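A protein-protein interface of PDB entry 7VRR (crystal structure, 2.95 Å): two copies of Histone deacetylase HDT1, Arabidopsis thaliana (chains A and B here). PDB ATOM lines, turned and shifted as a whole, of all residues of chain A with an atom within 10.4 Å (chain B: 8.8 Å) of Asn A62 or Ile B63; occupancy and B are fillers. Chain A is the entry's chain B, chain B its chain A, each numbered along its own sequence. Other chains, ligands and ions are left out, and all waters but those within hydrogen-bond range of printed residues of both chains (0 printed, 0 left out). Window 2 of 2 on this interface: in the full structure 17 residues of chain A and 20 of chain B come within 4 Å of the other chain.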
ATOM      1  N   LEU A  31      17.391  21.342 -25.090  1.00  0.00           N
ATOM      2  CA  LEU A  31      18.547  21.565 -25.967  1.00  0.00           C
ATOM      3  C   LEU A  31      19.795  21.811 -25.141  1.00  0.00           C
ATOM      4  O   LEU A  31      19.722  22.446 -24.104  1.00  0.00           O
ATOM      5  CB  LEU A  31      18.339  22.782 -26.860  1.00  0.00           C
ATOM      6  CG  LEU A  31      17.210  22.749 -27.912  1.00  0.00           C
ATOM      7  CD1 LEU A  31      17.254  23.983 -28.786  1.00  0.00           C
ATOM      8  CD2 LEU A  31      17.285  21.518 -28.777  1.00  0.00           C
ATOM      9  N   LYS A  38      22.602  30.304 -33.799  1.00  0.00           N
ATOM     10  CA  LYS A  38      21.632  30.117 -34.881  1.00  0.00           C
ATOM     11  C   LYS A  38      20.178  29.979 -34.360  1.00  0.00           C
ATOM     12  O   LYS A  38      19.948  29.419 -33.285  1.00  0.00           O
ATOM     13  CB  LYS A  38      22.018  28.888 -35.733  1.00  0.00           C
ATOM     14  CG  LYS A  38      21.299  28.776 -37.077  1.00  0.00           C
ATOM     15  CD  LYS A  38      21.533  27.398 -37.686  1.00  0.00           C
ATOM     16  CE  LYS A  38      20.689  27.141 -38.924  1.00  0.00           C
ATOM     17  NZ  LYS A  38      21.207  27.900 -40.099  1.00  0.00           N
ATOM     18  N   GLY A  39      19.220  30.507 -35.138  1.00  0.00           N
ATOM     19  CA  GLY A  39      17.780  30.219 -35.005  1.00  0.00           C
ATOM     20  C   GLY A  39      17.285  29.069 -35.905  1.00  0.00           C
ATOM     21  O   GLY A  39      17.322  29.188 -37.139  1.00  0.00           O
ATOM     22  N   GLU A  40      16.785  27.991 -35.287  1.00  0.00           N
ATOM     23  CA  GLU A  40      16.389  26.787 -35.990  1.00  0.00           C
ATOM     24  C   GLU A  40      15.507  25.851 -35.157  1.00  0.00           C
ATOM     25  O   GLU A  40      15.505  25.917 -33.937  1.00  0.00           O
ATOM     26  CB  GLU A  40      17.608  26.035 -36.541  1.00  0.00           C
ATOM     27  CG  GLU A  40      18.603  25.454 -35.536  1.00  0.00           C
ATOM     28  CD  GLU A  40      19.757  24.720 -36.227  1.00  0.00           C
ATOM     29  OE1 GLU A  40      19.504  23.979 -37.205  1.00  0.00           O
ATOM     30  OE2 GLU A  40      20.938  24.843 -35.784  1.00  0.00           O
ATOM     31  N   PHE A  41      14.781  24.965 -35.850  1.00  0.00           N
ATOM     32  CA  PHE A  41      13.785  24.063 -35.271  1.00  0.00           C
ATOM     33  C   PHE A  41      14.274  22.628 -35.185  1.00  0.00           C
ATOM     34  O   PHE A  41      14.971  22.159 -36.071  1.00  0.00           O
ATOM     35  CB  PHE A  41      12.491  24.131 -36.092  1.00  0.00           C
ATOM     36  CG  PHE A  41      11.683  25.370 -35.825  1.00  0.00           C
ATOM     37  CD1 PHE A  41      10.757  25.405 -34.777  1.00  0.00           C
ATOM     38  CD2 PHE A  41      11.894  26.527 -36.586  1.00  0.00           C
ATOM     39  CE1 PHE A  41      10.046  26.561 -34.501  1.00  0.00           C
ATOM     40  CE2 PHE A  41      11.173  27.679 -36.331  1.00  0.00           C
ATOM     41  CZ  PHE A  41      10.248  27.701 -35.290  1.00  0.00           C
ATOM     42  N   VAL A  42      13.856  21.931 -34.121  1.00  0.00           N
ATOM     43  CA  VAL A  42      14.324  20.591 -33.780  1.00  0.00           C
ATOM     44  C   VAL A  42      13.150  19.693 -33.396  1.00  0.00           C
ATOM     45  O   VAL A  42      12.742  19.637 -32.235  1.00  0.00           O
ATOM     46  CB  VAL A  42      15.306  20.636 -32.593  1.00  0.00           C
ATOM     47  CG1 VAL A  42      15.841  19.247 -32.267  1.00  0.00           C
ATOM     48  CG2 VAL A  42      16.439  21.623 -32.865  1.00  0.00           C
ATOM     49  N   THR A  57       8.476  19.937 -30.909  1.00  0.00           N
ATOM     50  CA  THR A  57       9.494  20.626 -31.662  1.00  0.00           C
ATOM     51  C   THR A  57      10.097  21.675 -30.759  1.00  0.00           C
ATOM     52  O   THR A  57       9.379  22.536 -30.245  1.00  0.00           O
ATOM     53  CB  THR A  57       8.887  21.289 -32.915  1.00  0.00           C
ATOM     54  OG1 THR A  57       8.079  20.333 -33.598  1.00  0.00           O
ATOM     55  CG2 THR A  57       9.967  21.773 -33.863  1.00  0.00           C
ATOM     56  N   LEU A  58      11.415  21.597 -30.553  1.00  0.00           N
ATOM     57  CA  LEU A  58      12.145  22.625 -29.822  1.00  0.00           C
ATOM     58  C   LEU A  58      12.640  23.665 -30.807  1.00  0.00           C
ATOM     59  O   LEU A  58      12.673  23.439 -32.001  1.00  0.00           O
ATOM     60  CB  LEU A  58      13.310  22.019 -29.027  1.00  0.00           C
ATOM     61  CG  LEU A  58      12.875  20.994 -27.983  1.00  0.00           C
ATOM     62  CD1 LEU A  58      14.069  20.272 -27.367  1.00  0.00           C
ATOM     63  CD2 LEU A  58      12.035  21.643 -26.906  1.00  0.00           C
ATOM     64  N   SER A  59      13.024  24.821 -30.281  1.00  0.00           N
ATOM     65  CA  SER A  59      13.481  25.944 -31.081  1.00  0.00           C
ATOM     66  C   SER A  59      14.587  26.642 -30.306  1.00  0.00           C
ATOM     67  O   SER A  59      14.445  26.907 -29.106  1.00  0.00           O
ATOM     68  CB  SER A  59      12.313  26.895 -31.378  1.00  0.00           C
ATOM     69  OG  SER A  59      12.703  28.253 -31.351  1.00  0.00           O
ATOM     70  N   THR A  60      15.692  26.934 -30.997  1.00  0.00           N
ATOM     71  CA  THR A  60      16.867  27.500 -30.346  1.00  0.00           C
ATOM     72  C   THR A  60      16.584  28.827 -29.628  1.00  0.00           C
ATOM     73  O   THR A  60      16.866  28.949 -28.437  1.00  0.00           O
ATOM     74  CB  THR A  60      18.051  27.642 -31.319  1.00  0.00           C
ATOM     75  OG1 THR A  60      17.656  28.396 -32.466  1.00  0.00           O
ATOM     76  CG2 THR A  60      18.527  26.275 -31.778  1.00  0.00           C
ATOM     77  N   GLU A  61      16.011  29.808 -30.333  1.00  0.00           N
ATOM     78  CA  GLU A  61      15.725  31.101 -29.732  1.00  0.00           C
ATOM     79  C   GLU A  61      14.520  31.104 -28.770  1.00  0.00           C
ATOM     80  O   GLU A  61      14.607  31.661 -27.682  1.00  0.00           O
ATOM     81  CB  GLU A  61      15.628  32.202 -30.801  1.00  0.00           C
ATOM     82  CG  GLU A  61      14.491  32.066 -31.799  1.00  0.00           C
ATOM     83  CD  GLU A  61      14.757  31.087 -32.940  1.00  0.00           C
ATOM     84  OE1 GLU A  61      14.711  29.845 -32.695  1.00  0.00           O
ATOM     85  OE2 GLU A  61      15.012  31.575 -34.081  1.00  0.00           O
ATOM     86  N   ASN A  62      13.413  30.458 -29.151  1.00  0.00           N
ATOM     87  CA  ASN A  62      12.139  30.551 -28.406  1.00  0.00           C
ATOM     88  C   ASN A  62      11.783  29.398 -27.472  1.00  0.00           C
ATOM     89  O   ASN A  62      11.164  29.638 -26.454  1.00  0.00           O
ATOM     90  CB  ASN A  62      10.975  30.681 -29.372  1.00  0.00           C
ATOM     91  CG  ASN A  62      11.187  31.737 -30.398  1.00  0.00           C
ATOM     92  OD1 ASN A  62      11.222  31.436 -31.590  1.00  0.00           O
ATOM     93  ND2 ASN A  62      11.364  32.975 -29.950  1.00  0.00           N
ATOM     94  N   ILE A  63      12.114  28.161 -27.857  1.00  0.00           N
ATOM     95  CA  ILE A  63      11.666  26.983 -27.128  1.00  0.00           C
ATOM     96  C   ILE A  63      12.832  26.048 -26.816  1.00  0.00           C
ATOM     97  O   ILE A  63      12.946  24.964 -27.378  1.00  0.00           O
ATOM     98  CB  ILE A  63      10.572  26.239 -27.908  1.00  0.00           C
ATOM     99  CG1 ILE A  63       9.440  27.187 -28.278  1.00  0.00           C
ATOM    100  CG2 ILE A  63       9.979  25.109 -27.076  1.00  0.00           C
ATOM    101  CD1 ILE A  63       8.487  26.619 -29.311  1.00  0.00           C
ATOM    102  N   PRO A  64      13.738  26.444 -25.898  1.00  0.00           N
ATOM    103  CA  PRO A  64      14.928  25.658 -25.590  1.00  0.00           C
ATOM    104  C   PRO A  64      14.625  24.307 -24.923  1.00  0.00           C
ATOM    105  O   PRO A  64      15.462  23.422 -24.993  1.00  0.00           O
ATOM    106  CB  PRO A  64      15.700  26.528 -24.589  1.00  0.00           C
ATOM    107  CG  PRO A  64      15.084  27.898 -24.694  1.00  0.00           C
ATOM    108  CD  PRO A  64      13.647  27.659 -25.084  1.00  0.00           C
ATOM    109  N   GLN A  65      13.468  24.199 -24.262  1.00  0.00           N
ATOM    110  CA  GLN A  65      13.048  22.963 -23.631  1.00  0.00           C
ATOM    111  C   GLN A  65      11.546  22.820 -23.687  1.00  0.00           C
ATOM    112  O   GLN A  65      10.833  23.785 -23.988  1.00  0.00           O
ATOM    113  CB  GLN A  65      13.523  22.899 -22.173  1.00  0.00           C
ATOM    114  CG  GLN A  65      13.085  24.062 -21.292  1.00  0.00           C
ATOM    115  CD  GLN A  65      14.006  25.264 -21.356  1.00  0.00           C
ATOM    116  OE1 GLN A  65      15.169  25.141 -21.684  1.00  0.00           O
ATOM    117  NE2 GLN A  65      13.488  26.432 -21.022  1.00  0.00           N
ATOM    118  N   LEU A  66      11.075  21.595 -23.432  1.00  0.00           N
ATOM    119  CA  LEU A  66       9.673  21.341 -23.166  1.00  0.00           C
ATOM    120  C   LEU A  66       9.514  20.361 -22.026  1.00  0.00           C
ATOM    121  O   LEU A  66      10.371  19.487 -21.783  1.00  0.00           O
ATOM    122  CB  LEU A  66       8.908  20.862 -24.403  1.00  0.00           C
ATOM    123  CG  LEU A  66       9.198  19.496 -25.019  1.00  0.00           C
ATOM    124  CD1 LEU A  66       8.720  18.331 -24.165  1.00  0.00           C
ATOM    125  CD2 LEU A  66       8.564  19.403 -26.389  1.00  0.00           C
ATOM    126  N   ALA B  29      12.739  26.102 -11.653  1.00  0.00           N
ATOM    127  CA  ALA B  29      13.957  26.883 -11.663  1.00  0.00           C
ATOM    128  C   ALA B  29      13.572  28.255 -12.135  1.00  0.00           C
ATOM    129  O   ALA B  29      12.919  28.391 -13.164  1.00  0.00           O
ATOM    130  CB  ALA B  29      14.965  26.275 -12.622  1.00  0.00           C
ATOM    131  N   SER B  30      13.996  29.274 -11.382  1.00  0.00           N
ATOM    132  CA  SER B  30      13.586  30.651 -11.602  1.00  0.00           C
ATOM    133  C   SER B  30      14.801  31.582 -11.426  1.00  0.00           C
ATOM    134  O   SER B  30      15.581  31.423 -10.498  1.00  0.00           O
ATOM    135  CB  SER B  30      12.429  31.014 -10.649  1.00  0.00           C
ATOM    136  OG  SER B  30      12.332  30.109  -9.538  1.00  0.00           O
ATOM    137  N   LEU B  31      14.955  32.535 -12.348  1.00  0.00           N
ATOM    138  CA  LEU B  31      15.962  33.581 -12.252  1.00  0.00           C
ATOM    139  C   LEU B  31      15.618  34.541 -11.118  1.00  0.00           C
ATOM    140  O   LEU B  31      14.452  34.825 -10.886  1.00  0.00           O
ATOM    141  CB  LEU B  31      16.021  34.395 -13.551  1.00  0.00           C
ATOM    142  CG  LEU B  31      16.519  33.750 -14.826  1.00  0.00           C
ATOM    143  CD1 LEU B  31      16.660  34.792 -15.924  1.00  0.00           C
ATOM    144  CD2 LEU B  31      17.846  33.018 -14.591  1.00  0.00           C
ATOM    145  N   GLU B  40      20.088  37.969 -21.705  1.00  0.00           N
ATOM    146  CA  GLU B  40      21.177  37.011 -21.386  1.00  0.00           C
ATOM    147  C   GLU B  40      20.637  35.590 -21.221  1.00  0.00           C
ATOM    148  O   GLU B  40      19.781  35.383 -20.339  1.00  0.00           O
ATOM    149  CB  GLU B  40      21.913  37.440 -20.116  1.00  0.00           C
ATOM    150  CG  GLU B  40      23.420  37.470 -20.281  1.00  0.00           C
ATOM    151  CD  GLU B  40      24.187  36.738 -19.195  1.00  0.00           C
ATOM    152  OE1 GLU B  40      24.843  37.416 -18.380  1.00  0.00           O
ATOM    153  OE2 GLU B  40      24.125  35.492 -19.166  1.00  0.00           O
ATOM    154  N   PHE B  41      21.119  34.651 -22.039  1.00  0.00           N
ATOM    155  CA  PHE B  41      20.744  33.240 -21.876  1.00  0.00           C
ATOM    156  C   PHE B  41      21.512  32.581 -20.734  1.00  0.00           C
ATOM    157  O   PHE B  41      22.695  32.858 -20.526  1.00  0.00           O
ATOM    158  CB  PHE B  41      21.016  32.492 -23.174  1.00  0.00           C
ATOM    159  CG  PHE B  41      19.981  32.732 -24.229  1.00  0.00           C
ATOM    160  CD1 PHE B  41      20.026  33.861 -25.069  1.00  0.00           C
ATOM    161  CD2 PHE B  41      18.956  31.816 -24.394  1.00  0.00           C
ATOM    162  CE1 PHE B  41      19.058  34.060 -26.031  1.00  0.00           C
ATOM    163  CE2 PHE B  41      17.984  32.002 -25.377  1.00  0.00           C
ATOM    164  CZ  PHE B  41      18.037  33.128 -26.186  1.00  0.00           C
ATOM    165  N   VAL B  42      20.828  31.675 -20.023  1.00  0.00           N
ATOM    166  CA  VAL B  42      21.339  31.036 -18.817  1.00  0.00           C
ATOM    167  C   VAL B  42      21.081  29.533 -18.841  1.00  0.00           C
ATOM    168  O   VAL B  42      20.028  29.072 -18.403  1.00  0.00           O
ATOM    169  CB  VAL B  42      20.679  31.619 -17.544  1.00  0.00           C
ATOM    170  CG1 VAL B  42      21.329  31.025 -16.295  1.00  0.00           C
ATOM    171  CG2 VAL B  42      20.747  33.140 -17.546  1.00  0.00           C
ATOM    172  N   LEU B  44      21.154  25.839 -17.452  1.00  0.00           N
ATOM    173  CA  LEU B  44      21.119  25.196 -16.158  1.00  0.00           C
ATOM    174  C   LEU B  44      21.736  23.814 -16.278  1.00  0.00           C
ATOM    175  O   LEU B  44      21.288  23.003 -17.083  1.00  0.00           O
ATOM    176  CB  LEU B  44      19.669  25.087 -15.680  1.00  0.00           C
ATOM    177  CG  LEU B  44      18.898  26.400 -15.689  1.00  0.00           C
ATOM    178  CD1 LEU B  44      17.484  26.152 -15.193  1.00  0.00           C
ATOM    179  CD2 LEU B  44      19.607  27.454 -14.865  1.00  0.00           C
ATOM    180  N   GLY B  56      17.856  22.872 -18.873  1.00  0.00           N
ATOM    181  CA  GLY B  56      17.133  23.893 -19.591  1.00  0.00           C
ATOM    182  C   GLY B  56      17.953  25.137 -19.720  1.00  0.00           C
ATOM    183  O   GLY B  56      19.036  25.215 -19.185  1.00  0.00           O
ATOM    184  N   THR B  57      17.421  26.104 -20.468  1.00  0.00           N
ATOM    185  CA  THR B  57      18.037  27.398 -20.658  1.00  0.00           C
ATOM    186  C   THR B  57      16.988  28.448 -20.345  1.00  0.00           C
ATOM    187  O   THR B  57      15.921  28.461 -20.953  1.00  0.00           O
ATOM    188  CB  THR B  57      18.539  27.557 -22.086  1.00  0.00           C
ATOM    189  OG1 THR B  57      19.257  26.382 -22.454  1.00  0.00           O
ATOM    190  CG2 THR B  57      19.435  28.787 -22.213  1.00  0.00           C
ATOM    191  N   LEU B  58      17.282  29.299 -19.357  1.00  0.00           N
ATOM    192  CA  LEU B  58      16.422  30.417 -19.025  1.00  0.00           C
ATOM    193  C   LEU B  58      16.885  31.625 -19.818  1.00  0.00           C
ATOM    194  O   LEU B  58      17.992  31.649 -20.365  1.00  0.00           O
ATOM    195  CB  LEU B  58      16.447  30.697 -17.528  1.00  0.00           C
ATOM    196  CG  LEU B  58      15.938  29.524 -16.670  1.00  0.00           C
ATOM    197  CD1 LEU B  58      16.172  29.754 -15.181  1.00  0.00           C
ATOM    198  CD2 LEU B  58      14.462  29.257 -16.938  1.00  0.00           C
ATOM    199  N   SER B  59      16.006  32.623 -19.901  1.00  0.00           N
ATOM    200  CA  SER B  59      16.269  33.836 -20.644  1.00  0.00           C
ATOM    201  C   SER B  59      15.696  35.006 -19.862  1.00  0.00           C
ATOM    202  O   SER B  59      14.551  34.947 -19.392  1.00  0.00           O
ATOM    203  CB  SER B  59      15.651  33.737 -22.040  1.00  0.00           C
ATOM    204  OG  SER B  59      15.091  34.979 -22.483  1.00  0.00           O
ATOM    205  N   THR B  60      16.508  36.060 -19.719  1.00  0.00           N
ATOM    206  CA  THR B  60      16.132  37.205 -18.890  1.00  0.00           C
ATOM    207  C   THR B  60      14.810  37.866 -19.315  1.00  0.00           C
ATOM    208  O   THR B  60      13.907  37.994 -18.499  1.00  0.00           O
ATOM    209  CB  THR B  60      17.268  38.242 -18.792  1.00  0.00           C
ATOM    210  OG1 THR B  60      17.673  38.643 -20.098  1.00  0.00           O
ATOM    211  CG2 THR B  60      18.464  37.643 -18.063  1.00  0.00           C
ATOM    212  N   GLU B  61      14.689  38.256 -20.588  1.00  0.00           N
ATOM    213  CA  GLU B  61      13.482  38.918 -21.063  1.00  0.00           C
ATOM    214  C   GLU B  61      12.276  37.964 -21.246  1.00  0.00           C
ATOM    215  O   GLU B  61      11.165  38.289 -20.830  1.00  0.00           O
ATOM    216  CB  GLU B  61      13.765  39.756 -22.321  1.00  0.00           C
ATOM    217  CG  GLU B  61      14.205  38.985 -23.556  1.00  0.00           C
ATOM    218  CD  GLU B  61      15.699  38.611 -23.555  1.00  0.00           C
ATOM    219  OE1 GLU B  61      16.091  37.665 -22.811  1.00  0.00           O
ATOM    220  OE2 GLU B  61      16.488  39.256 -24.300  1.00  0.00           O
ATOM    221  N   ASN B  62      12.496  36.784 -21.851  1.00  0.00           N
ATOM    222  CA  ASN B  62      11.416  35.885 -22.274  1.00  0.00           C
ATOM    223  C   ASN B  62      11.105  34.691 -21.399  1.00  0.00           C
ATOM    224  O   ASN B  62       9.949  34.296 -21.327  1.00  0.00           O
ATOM    225  CB  ASN B  62      11.719  35.334 -23.652  1.00  0.00           C
ATOM    226  CG  ASN B  62      11.955  36.416 -24.658  1.00  0.00           C
ATOM    227  OD1 ASN B  62      11.349  37.500 -24.588  1.00  0.00           O
ATOM    228  ND2 ASN B  62      12.856  36.153 -25.595  1.00  0.00           N
ATOM    229  N   ILE B  63      12.130  34.078 -20.793  1.00  0.00           N
ATOM    230  CA  ILE B  63      11.955  32.832 -20.056  1.00  0.00           C
ATOM    231  C   ILE B  63      12.555  32.932 -18.656  1.00  0.00           C
ATOM    232  O   ILE B  63      13.566  32.306 -18.357  1.00  0.00           O
ATOM    233  CB  ILE B  63      12.553  31.651 -20.827  1.00  0.00           C
ATOM    234  CG1 ILE B  63      11.974  31.599 -22.234  1.00  0.00           C
ATOM    235  CG2 ILE B  63      12.234  30.331 -20.137  1.00  0.00           C
ATOM    236  CD1 ILE B  63      12.663  30.628 -23.160  1.00  0.00           C
ATOM    237  N   PRO B  64      11.939  33.724 -17.752  1.00  0.00           N
ATOM    238  CA  PRO B  64      12.479  33.945 -16.414  1.00  0.00           C
ATOM    239  C   PRO B  64      12.475  32.687 -15.535  1.00  0.00           C
ATOM    240  O   PRO B  64      13.233  32.641 -14.593  1.00  0.00           O
ATOM    241  CB  PRO B  64      11.527  34.976 -15.791  1.00  0.00           C
ATOM    242  CG  PRO B  64      10.744  35.548 -16.947  1.00  0.00           C
ATOM    243  CD  PRO B  64      10.674  34.435 -17.959  1.00  0.00           C
ATOM    244  N   GLN B  65      11.597  31.730 -15.836  1.00  0.00           N
ATOM    245  CA  GLN B  65      11.527  30.481 -15.099  1.00  0.00           C
ATOM    246  C   GLN B  65      11.130  29.344 -16.017  1.00  0.00           C
ATOM    247  O   GLN B  65      10.678  29.566 -17.145  1.00  0.00           O
ATOM    248  CB  GLN B  65      10.526  30.590 -13.939  1.00  0.00           C
ATOM    249  CG  GLN B  65       9.110  30.998 -14.332  1.00  0.00           C
ATOM    250  CD  GLN B  65       8.909  32.493 -14.416  1.00  0.00           C
ATOM    251  OE1 GLN B  65       9.633  33.249 -13.773  1.00  0.00           O
ATOM    252  NE2 GLN B  65       7.913  32.930 -15.200  1.00  0.00           N
ATOM    253  N   LEU B  66      11.330  28.122 -15.521  1.00  0.00           N
ATOM    254  CA  LEU B  66      10.742  26.935 -16.106  1.00  0.00           C
ATOM    255  C   LEU B  66      10.211  26.006 -15.039  1.00  0.00           C
ATOM    256  O   LEU B  66      10.703  25.971 -13.888  1.00  0.00           O
ATOM    257  CB  LEU B  66      11.734  26.203 -17.012  1.00  0.00           C
ATOM    258  CG  LEU B  66      12.971  25.530 -16.442  1.00  0.00           C
ATOM    259  CD1 LEU B  66      12.643  24.269 -15.669  1.00  0.00           C
ATOM    260  CD2 LEU B  66      13.922  25.203 -17.573  1.00  0.00           C
ATOM    261  N   PHE B  67       9.195  25.244 -15.440  1.00  0.00           N
ATOM    262  CA  PHE B  67       8.534  24.269 -14.604  1.00  0.00           C
ATOM    263  C   PHE B  67       9.080  22.871 -14.936  1.00  0.00           C
ATOM    264  O   PHE B  67       9.389  22.571 -16.102  1.00  0.00           O
ATOM    265  CB  PHE B  67       7.033  24.354 -14.855  1.00  0.00           C
ATOM    266  CG  PHE B  67       6.285  23.219 -14.287  1.00  0.00           C
ATOM    267  CD1 PHE B  67       5.951  23.206 -12.949  1.00  0.00           C
ATOM    268  CD2 PHE B  67       5.968  22.127 -15.068  1.00  0.00           C
ATOM    269  CE1 PHE B  67       5.284  22.134 -12.401  1.00  0.00           C
ATOM    270  CE2 PHE B  67       5.313  21.048 -14.523  1.00  0.00           C
ATOM    271  CZ  PHE B  67       4.967  21.050 -13.192  1.00  0.00           C
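Asn A62 touches Ile B63.
CG of Pro A64 touches O of Thr B57 (3.9 Å).
Pro A64 touches Ile B63.
Gly B56 touches Gln A65 (CA to OE1, 3.1 Å).
Gln A65 touches Leu B66 (NE2 to CD2, 3.7 Å).
Along chain A the printed residues that touch a printed residue of chain B span positions 62 to 65.
Hydrophobic or aromatic side chains of chain B within 4 Å of the printed part of chain A: Ile B63 and Leu B66.
Along chain B the printed residues that touch a printed residue of chain A span positions 56 to 66.
Among the printed residues, 6 pairs touch across the chains.
Among the printed residues, no Asp or Glu carboxylate lies within 4 Å of a Lys or Arg side-chain nitrogen of the other chain.
O of Ala B29 is in hydrogen-bond range of N of Leu B66 (2.9 Å).
The backbone NH (N) of Leu B44 is in hydrogen-bond range of the backbone carbonyl oxygen (O) of Gly B56 (2.8 Å).
The backbone NH (N) of Leu A31 lies within hydrogen-bond range of the backbone carbonyl oxygen (O) of Pro A64, 2.8 Å away.
The side-chain hydroxyl (OG) of Ser A59 lies within hydrogen-bond range of the backbone NH (N) of Asn A62, 3.2 Å away.
Asn A62 touches Ile B63, but with the chains exchanged Ile A63 does not touch Asn B62 (8.3 Å).
Pro A64 touches Thr B57, but with the chains exchanged Thr A57 does not touch Pro B64 (17.0 Å).
Pro A64 touches Ile B63, but with the chains exchanged Ile A63 does not touch Pro B64 (11.5 Å).
Gln A65 touches Leu B66, but with the chains exchanged Leu A66 does not touch Gln B65 (10.2 Å).
Of the 6 pairs that touch across the chains among the printed residues, none has its exchanged pair printed and touching as well.
The side-chain amide oxygen of Gln A65 lies within hydrogen-bond range of the backbone NH of Thr B57 (2.7 Å).
Leu A58 touches none of the printed residues of chain B.
Asn A62 touches one residue of chain B.
No residue of chain B comes within 4 Å of Ile A63.
Of the printed residues of chain B, Pro A64 touches Thr B57 and Ile B63.
Of the printed residues of chain B, Gln A65 touches Gly B56, Thr B57 and Leu B66.
Printed residues of chain A within 4 Å of Gly B56: Gln A65 (3.1 Å).
No residue of chain A comes within 4 Å of Leu B58.
Ser B59 touches none of the printed residues of chain A.
Of chain A, only Asn A62 (3.8 Å) and Pro A64 (3.7 Å) come within 4 Å of Ile B63.
No residue of chain A comes within 4 Å of Pro B64.
No residue of chain A comes within 4 Å of Gln B65.
Of the printed residues of chain A, Leu B66 touches Gln A65 (3.7 Å).
The nearest printed residue of chain B that does not touch Gln A65 is Ile B63 (4.2 Å).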
